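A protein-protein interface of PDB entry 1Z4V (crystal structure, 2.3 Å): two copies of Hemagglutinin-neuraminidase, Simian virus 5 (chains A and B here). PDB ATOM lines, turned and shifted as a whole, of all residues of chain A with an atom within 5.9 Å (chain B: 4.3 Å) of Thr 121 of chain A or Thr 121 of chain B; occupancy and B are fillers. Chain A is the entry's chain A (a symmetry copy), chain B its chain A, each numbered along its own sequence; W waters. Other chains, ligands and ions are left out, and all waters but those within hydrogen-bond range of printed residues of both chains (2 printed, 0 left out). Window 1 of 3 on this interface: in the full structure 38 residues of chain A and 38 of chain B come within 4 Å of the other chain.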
ATOM      1  N   ASN A 114     -33.407   0.145 -21.392  1.00  0.00           N
ATOM      2  CA  ASN A 114     -32.940   1.435 -20.887  1.00  0.00           C
ATOM      3  C   ASN A 114     -33.792   2.054 -19.794  1.00  0.00           C
ATOM      4  O   ASN A 114     -34.938   2.420 -20.016  1.00  0.00           O
ATOM      5  CB  ASN A 114     -32.813   2.451 -22.021  1.00  0.00           C
ATOM      6  CG  ASN A 114     -32.231   3.778 -21.545  1.00  0.00           C
ATOM      7  OD1 ASN A 114     -31.064   3.831 -21.127  1.00  0.00           O
ATOM      8  ND2 ASN A 114     -33.006   4.821 -21.586  1.00  0.00           N
ATOM      9  N   MET A 115     -33.201   2.184 -18.613  1.00  0.00           N
ATOM     10  CA  MET A 115     -33.869   2.798 -17.481  1.00  0.00           C
ATOM     11  C   MET A 115     -32.900   3.820 -16.902  1.00  0.00           C
ATOM     12  O   MET A 115     -31.697   3.738 -17.143  1.00  0.00           O
ATOM     13  CB  MET A 115     -34.212   1.748 -16.416  1.00  0.00           C
ATOM     14  CG  MET A 115     -33.012   1.093 -15.795  1.00  0.00           C
ATOM     15  SD  MET A 115     -33.443   0.004 -14.421  1.00  0.00           S
ATOM     16  CE  MET A 115     -31.802  -0.288 -13.731  1.00  0.00           C
ATOM     17  N   PRO A 116     -33.411   4.821 -16.168  1.00  0.00           N
ATOM     18  CA  PRO A 116     -32.506   5.815 -15.585  1.00  0.00           C
ATOM     19  C   PRO A 116     -31.689   5.108 -14.506  1.00  0.00           C
ATOM     20  O   PRO A 116     -32.246   4.525 -13.576  1.00  0.00           O
ATOM     21  CB  PRO A 116     -33.460   6.852 -14.989  1.00  0.00           C
ATOM     22  CG  PRO A 116     -34.699   6.711 -15.837  1.00  0.00           C
ATOM     23  CD  PRO A 116     -34.814   5.218 -15.986  1.00  0.00           C
ATOM     24  N   SER A 117     -30.371   5.142 -14.634  1.00  0.00           N
ATOM     25  CA  SER A 117     -29.508   4.495 -13.664  1.00  0.00           C
ATOM     26  C   SER A 117     -29.622   5.118 -12.271  1.00  0.00           C
ATOM     27  O   SER A 117     -29.679   6.334 -12.141  1.00  0.00           O
ATOM     28  CB  SER A 117     -28.054   4.578 -14.121  1.00  0.00           C
ATOM     29  OG  SER A 117     -27.198   3.979 -13.155  1.00  0.00           O
ATOM     30  N   ILE A 119     -27.282   4.439 -10.014  1.00  0.00           N
ATOM     31  CA  ILE A 119     -25.905   4.410  -9.527  1.00  0.00           C
ATOM     32  C   ILE A 119     -25.180   5.647 -10.053  1.00  0.00           C
ATOM     33  O   ILE A 119     -24.998   5.803 -11.253  1.00  0.00           O
ATOM     34  CB  ILE A 119     -25.181   3.127  -9.999  1.00  0.00           C
ATOM     35  CG1 ILE A 119     -25.960   1.898  -9.513  1.00  0.00           C
ATOM     36  CG2 ILE A 119     -23.764   3.098  -9.468  1.00  0.00           C
ATOM     37  CD1 ILE A 119     -25.355   0.577  -9.909  1.00  0.00           C
ATOM     38  N   PRO A 120     -24.761   6.544  -9.151  1.00  0.00           N
ATOM     39  CA  PRO A 120     -24.071   7.773  -9.539  1.00  0.00           C
ATOM     40  C   PRO A 120     -22.726   7.586 -10.226  1.00  0.00           C
ATOM     41  O   PRO A 120     -21.945   6.696  -9.897  1.00  0.00           O
ATOM     42  CB  PRO A 120     -23.957   8.534  -8.218  1.00  0.00           C
ATOM     43  CG  PRO A 120     -23.753   7.425  -7.236  1.00  0.00           C
ATOM     44  CD  PRO A 120     -24.785   6.395  -7.683  1.00  0.00           C
ATOM     45  N   THR A 121     -22.472   8.473 -11.167  1.00  0.00           N
ATOM     46  CA  THR A 121     -21.256   8.517 -11.971  1.00  0.00           C
ATOM     47  C   THR A 121     -20.242   9.521 -11.386  1.00  0.00           C
ATOM     48  O   THR A 121     -20.610  10.394 -10.603  1.00  0.00           O
ATOM     49  CB  THR A 121     -21.648   8.932 -13.420  1.00  0.00           C
ATOM     50  OG1 THR A 121     -21.978   7.756 -14.171  1.00  0.00           O
ATOM     51  CG2 THR A 121     -20.558   9.679 -14.100  1.00  0.00           C
ATOM     52  N   ALA A 122     -18.975   9.381 -11.765  1.00  0.00           N
ATOM     53  CA  ALA A 122     -17.932  10.288 -11.313  1.00  0.00           C
ATOM     54  C   ALA A 122     -18.023  11.536 -12.198  1.00  0.00           C
ATOM     55  O   ALA A 122     -18.598  11.470 -13.282  1.00  0.00           O
ATOM     56  CB  ALA A 122     -16.570   9.629 -11.463  1.00  0.00           C
ATOM     57  N   THR A 123     -17.477  12.665 -11.745  1.00  0.00           N
ATOM     58  CA  THR A 123     -17.536  13.890 -12.542  1.00  0.00           C
ATOM     59  C   THR A 123     -16.171  14.400 -12.999  1.00  0.00           C
ATOM     60  O   THR A 123     -16.047  15.532 -13.472  1.00  0.00           O
ATOM     61  CB  THR A 123     -18.266  15.025 -11.778  1.00  0.00           C
ATOM     62  OG1 THR A 123     -17.679  15.189 -10.476  1.00  0.00           O
ATOM     63  CG2 THR A 123     -19.745  14.697 -11.628  1.00  0.00           C
ATOM     64  N   THR A 129     -14.993   5.162  -8.775  1.00  0.00           N
ATOM     65  CA  THR A 129     -16.136   4.600  -8.063  1.00  0.00           C
ATOM     66  C   THR A 129     -16.017   3.090  -8.212  1.00  0.00           C
ATOM     67  O   THR A 129     -16.019   2.576  -9.328  1.00  0.00           O
ATOM     68  CB  THR A 129     -17.485   5.063  -8.666  1.00  0.00           C
ATOM     69  OG1 THR A 129     -17.566   4.694 -10.047  1.00  0.00           O
ATOM     70  CG2 THR A 129     -17.628   6.576  -8.558  1.00  0.00           C
ATOM     71  N   HIS A 145     -21.446   2.164  -2.821  1.00  0.00           N
ATOM     72  CA  HIS A 145     -20.154   1.954  -3.461  1.00  0.00           C
ATOM     73  C   HIS A 145     -19.129   2.954  -2.921  1.00  0.00           C
ATOM     74  O   HIS A 145     -19.483   3.980  -2.328  1.00  0.00           O
ATOM     75  CB  HIS A 145     -20.253   1.987  -5.002  1.00  0.00           C
ATOM     76  CG  HIS A 145     -20.482   3.333  -5.605  1.00  0.00           C
ATOM     77  ND1 HIS A 145     -21.245   3.516  -6.733  1.00  0.00           N
ATOM     78  CD2 HIS A 145     -19.977   4.560  -5.296  1.00  0.00           C
ATOM     79  CE1 HIS A 145     -21.207   4.787  -7.101  1.00  0.00           C
ATOM     80  NE2 HIS A 145     -20.438   5.436  -6.239  1.00  0.00           N
ATOM     81  N   LEU A 517     -15.757   9.730 -18.397  1.00  0.00           N
ATOM     82  CA  LEU A 517     -15.787  10.161 -16.997  1.00  0.00           C
ATOM     83  C   LEU A 517     -15.441   9.055 -16.010  1.00  0.00           C
ATOM     84  O   LEU A 517     -16.033   7.977 -16.040  1.00  0.00           O
ATOM     85  CB  LEU A 517     -17.165  10.732 -16.647  1.00  0.00           C
ATOM     86  CG  LEU A 517     -17.454  12.195 -17.012  1.00  0.00           C
ATOM     87  CD1 LEU A 517     -16.489  13.103 -16.269  1.00  0.00           C
ATOM     88  CD2 LEU A 517     -17.316  12.400 -18.504  1.00  0.00           C
ATOM     89  N   GLN A 521     -17.252   3.130 -14.483  1.00  0.00           N
ATOM     90  CA  GLN A 521     -18.621   3.592 -14.469  1.00  0.00           C
ATOM     91  C   GLN A 521     -19.337   2.322 -14.045  1.00  0.00           C
ATOM     92  O   GLN A 521     -19.284   1.309 -14.750  1.00  0.00           O
ATOM     93  CB  GLN A 521     -19.103   4.026 -15.853  1.00  0.00           C
ATOM     94  CG  GLN A 521     -20.459   4.738 -15.799  1.00  0.00           C
ATOM     95  CD  GLN A 521     -20.983   5.167 -17.166  1.00  0.00           C
ATOM     96  OE1 GLN A 521     -20.227   5.617 -18.019  1.00  0.00           O
ATOM     97  NE2 GLN A 521     -22.287   5.045 -17.365  1.00  0.00           N
ATOM     98  N   ILE A 522     -19.945   2.344 -12.869  1.00  0.00           N
ATOM     99  CA  ILE A 522     -20.681   1.180 -12.389  1.00  0.00           C
ATOM    100  C   ILE A 522     -22.071   1.279 -13.017  1.00  0.00           C
ATOM    101  O   ILE A 522     -22.823   2.215 -12.757  1.00  0.00           O
ATOM    102  CB  ILE A 522     -20.755   1.178 -10.862  1.00  0.00           C
ATOM    103  CG1 ILE A 522     -19.333   1.053 -10.298  1.00  0.00           C
ATOM    104  CG2 ILE A 522     -21.615   0.023 -10.376  1.00  0.00           C
ATOM    105  CD1 ILE A 522     -19.247   1.045  -8.780  1.00  0.00           C
ATOM    106  N   VAL A 523     -22.399   0.317 -13.866  1.00  0.00           N
ATOM    107  CA  VAL A 523     -23.658   0.325 -14.586  1.00  0.00           C
ATOM    108  C   VAL A 523     -24.633  -0.763 -14.155  1.00  0.00           C
ATOM    109  O   VAL A 523     -24.262  -1.926 -14.012  1.00  0.00           O
ATOM    110  CB  VAL A 523     -23.403   0.165 -16.104  1.00  0.00           C
ATOM    111  CG1 VAL A 523     -24.726   0.151 -16.865  1.00  0.00           C
ATOM    112  CG2 VAL A 523     -22.503   1.293 -16.603  1.00  0.00           C
ATOM    113  N   MET B 115     -17.474  14.584  -7.648  1.00  0.00           N
ATOM    114  CA  MET B 115     -18.566  14.376  -6.716  1.00  0.00           C
ATOM    115  C   MET B 115     -19.491  13.344  -7.347  1.00  0.00           C
ATOM    116  O   MET B 115     -19.456  13.141  -8.559  1.00  0.00           O
ATOM    117  CB  MET B 115     -19.334  15.682  -6.476  1.00  0.00           C
ATOM    118  CG  MET B 115     -20.023  16.219  -7.698  1.00  0.00           C
ATOM    119  SD  MET B 115     -21.066  17.649  -7.343  1.00  0.00           S
ATOM    120  CE  MET B 115     -21.967  17.770  -8.901  1.00  0.00           C
ATOM    121  N   PRO B 116     -20.300  12.648  -6.532  1.00  0.00           N
ATOM    122  CA  PRO B 116     -21.211  11.655  -7.107  1.00  0.00           C
ATOM    123  C   PRO B 116     -22.264  12.417  -7.910  1.00  0.00           C
ATOM    124  O   PRO B 116     -22.953  13.287  -7.378  1.00  0.00           O
ATOM    125  CB  PRO B 116     -21.815  10.978  -5.876  1.00  0.00           C
ATOM    126  CG  PRO B 116     -20.750  11.159  -4.823  1.00  0.00           C
ATOM    127  CD  PRO B 116     -20.302  12.575  -5.065  1.00  0.00           C
ATOM    128  N   SER B 117     -22.379  12.105  -9.193  1.00  0.00           N
ATOM    129  CA  SER B 117     -23.346  12.775 -10.041  1.00  0.00           C
ATOM    130  C   SER B 117     -24.789  12.512  -9.606  1.00  0.00           C
ATOM    131  O   SER B 117     -25.136  11.390  -9.263  1.00  0.00           O
ATOM    132  CB  SER B 117     -23.178  12.319 -11.487  1.00  0.00           C
ATOM    133  OG  SER B 117     -24.148  12.944 -12.319  1.00  0.00           O
ATOM    134  N   ILE B 119     -27.254  13.220 -11.718  1.00  0.00           N
ATOM    135  CA  ILE B 119     -27.963  13.095 -12.989  1.00  0.00           C
ATOM    136  C   ILE B 119     -27.818  11.657 -13.483  1.00  0.00           C
ATOM    137  O   ILE B 119     -26.721  11.206 -13.784  1.00  0.00           O
ATOM    138  CB  ILE B 119     -27.391  14.079 -14.037  1.00  0.00           C
ATOM    139  CG1 ILE B 119     -27.489  15.510 -13.494  1.00  0.00           C
ATOM    140  CG2 ILE B 119     -28.149  13.956 -15.341  1.00  0.00           C
ATOM    141  CD1 ILE B 119     -26.963  16.570 -14.425  1.00  0.00           C
ATOM    142  N   PRO B 120     -28.934  10.921 -13.569  1.00  0.00           N
ATOM    143  CA  PRO B 120     -28.914   9.529 -14.012  1.00  0.00           C
ATOM    144  C   PRO B 120     -28.453   9.299 -15.445  1.00  0.00           C
ATOM    145  O   PRO B 120     -28.740  10.075 -16.353  1.00  0.00           O
ATOM    146  CB  PRO B 120     -30.355   9.073 -13.777  1.00  0.00           C
ATOM    147  CG  PRO B 120     -31.128  10.314 -14.090  1.00  0.00           C
ATOM    148  CD  PRO B 120     -30.318  11.396 -13.383  1.00  0.00           C
ATOM    149  N   THR B 121     -27.758   8.193 -15.617  1.00  0.00           N
ATOM    150  CA  THR B 121     -27.204   7.740 -16.888  1.00  0.00           C
ATOM    151  C   THR B 121     -28.140   6.718 -17.566  1.00  0.00           C
ATOM    152  O   THR B 121     -28.997   6.128 -16.912  1.00  0.00           O
ATOM    153  CB  THR B 121     -25.815   7.094 -16.610  1.00  0.00           C
ATOM    154  OG1 THR B 121     -24.808   8.114 -16.653  1.00  0.00           O
ATOM    155  CG2 THR B 121     -25.493   6.022 -17.587  1.00  0.00           C
ATOM    156  N   ALA B 122     -27.972   6.527 -18.871  1.00  0.00           N
ATOM    157  CA  ALA B 122     -28.764   5.562 -19.616  1.00  0.00           C
ATOM    158  C   ALA B 122     -28.131   4.189 -19.368  1.00  0.00           C
ATOM    159  O   ALA B 122     -26.970   4.119 -18.972  1.00  0.00           O
ATOM    160  CB  ALA B 122     -28.736   5.899 -21.099  1.00  0.00           C
ATOM    161  N   THR B 123     -28.880   3.106 -19.584  1.00  0.00           N
ATOM    162  CA  THR B 123     -28.332   1.769 -19.360  1.00  0.00           C
ATOM    163  C   THR B 123     -28.229   0.920 -20.625  1.00  0.00           C
ATOM    164  O   THR B 123     -28.009  -0.292 -20.555  1.00  0.00           O
ATOM    165  CB  THR B 123     -29.156   0.993 -18.299  1.00  0.00           C
ATOM    166  OG1 THR B 123     -30.548   1.014 -18.657  1.00  0.00           O
ATOM    167  CG2 THR B 123     -28.977   1.620 -16.924  1.00  0.00           C
ATOM    168  N   GLN B 521     -24.464  11.570 -22.290  1.00  0.00           N
ATOM    169  CA  GLN B 521     -24.322  11.392 -20.863  1.00  0.00           C
ATOM    170  C   GLN B 521     -24.364  12.836 -20.398  1.00  0.00           C
ATOM    171  O   GLN B 521     -23.501  13.638 -20.769  1.00  0.00           O
ATOM    172  CB  GLN B 521     -22.984  10.760 -20.485  1.00  0.00           C
ATOM    173  CG  GLN B 521     -22.931  10.348 -19.009  1.00  0.00           C
ATOM    174  CD  GLN B 521     -21.600   9.734 -18.590  1.00  0.00           C
ATOM    175  OE1 GLN B 521     -20.995   8.970 -19.334  1.00  0.00           O
ATOM    176  NE2 GLN B 521     -21.154  10.053 -17.385  1.00  0.00           N
HETATM  177  O   HOH W   1     -26.237   7.294 -13.221  1.00  0.00           O
HETATM  178  O   HOH W   2     -24.885   9.578 -12.517  1.00  0.00           O
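Printed residues of chain B within 4 Å of Asn 114 of chain A: Ala 122 and Thr 123.
Thr 121 of chain A touches just these residues of chain B: Met 115 (3.6 Å), Pro 116 (3.8 Å), Ser 117 (2.8 Å), Thr 121 (3.8 Å) and Gln 521 (3.4 Å).
Printed residues of chain B within 4 Å of Gln 521 of chain A: Thr 121 and Gln 521.
Val 523 of chain A touches none of the printed residues of chain B.
Of the printed residues of chain A, Met 115 of chain B touches Thr 121 (3.6 Å) and Thr 123 (2.9 Å).
Of the printed residues of chain A, Thr 121 of chain B touches Met 115, Pro 116, Ser 117, Thr 121 and Gln 521.
Of the printed residues of chain A, Gln 521 of chain B touches Thr 121 and Gln 521.
The nearest printed residue of chain B that does not touch Thr 121 of chain A is Ile 119 of chain B (5.6 Å).
The nearest residue of chain A that does not touch Thr 121 of chain B is Asn 114 of chain A (5.2 Å).
The nearest printed residue of chain A that does not touch Pro 116 of chain B is Pro 120 of chain A (4.01 Å).
Hydrophobic or aromatic side chains of chain A within 4 Å of the printed part of chain B: Met 115 and Pro 120.
Printed residues of chain B that touch a printed residue of chain A: Met 115, Pro 116, Ser 117, Pro 120, Thr 121, Ala 122, Thr 123 and Gln 521.
Hydrophobic or aromatic side chains of chain B that line the printed part of chain A: Met 115, Pro 120 and Ala 122.
Among the printed residues, no Asp or Glu carboxylate lies within 4 Å of a Lys or Arg side-chain nitrogen of the other chain.
The backbone NH (N) of Ile 119 of chain B lies within hydrogen-bond range of the side-chain hydroxyl (OG) of Ser 117 of chain B (3.2 Å).
The backbone NH of Ile 119 of chain A lies within hydrogen-bond range of the side-chain hydroxyl of Ser 117 of chain A (3.2 Å).
Among the printed residues, merely in contact across the chains: Asn 114 of chain A with Ala 122 of chain B, Met 115 of chain A with Thr 121 of chain B, Pro 116 of chain A with Thr 121 of chain B, Ser 117 of chain A with Pro 120 of chain B, Pro 120 of chain A with Ser 117 of chain B, Thr 121 of chain A with Met 115 of chain B, Thr 121 of chain A with Pro 116 of chain B, Thr 121 of chain A with Thr 121 of chain B, Thr 121 of chain A with Gln 521 of chain B, Gln 521 of chain A with Thr 121 of chain B and Gln 521 of chain A with Gln 521 of chain B.
Water W2 lies within hydrogen-bond range of O of Ile 119 of chain B (2.8 Å), N of Thr 121 of chain A (3.0 Å) and OG of Ser 117 of chain B (3.5 Å).
Water W1 lies within hydrogen-bond range of O of Ile 119 of chain A, N of Thr 121 of chain B and OG of Ser 117 of chain A.
Ser 117 of chain A touches Pro 120 of chain B, and with the chains exchanged Pro 120 of chain A touches Ser 117 of chain B.
Ser 117 of chain A touches Thr 121 of chain B, and with the chains exchanged Thr 121 of chain A touches Ser 117 of chain B.
Thr 121 of chain A touches its own counterpart, Thr 121 of chain B.
Gln 521 of chain B touches its own counterpart, Gln 521 of chain A.
The side-chain amide oxygen of Asn 114 of chain A lies within hydrogen-bond range of the backbone NH of Thr 123 of chain B.
The backbone NH (N) of Met 115 of chain A is in hydrogen-bond range of the side-chain hydroxyl (OG1) of Thr 123 of chain B, at 2.9 Å.
N of Met 115 of chain B lies within hydrogen-bond range of OG1 of Thr 123 of chain A (2.9 Å).
The backbone NH (N) of Ser 117 of chain B sits at hydrogen-bond distance from the backbone carbonyl oxygen (O) of Thr 121 of chain A (2.8 Å).
The backbone carbonyl oxygen (O) of Thr 121 of chain B sits at hydrogen-bond distance from the backbone NH (N) of Ser 117 of chain A, 2.8 Å away.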
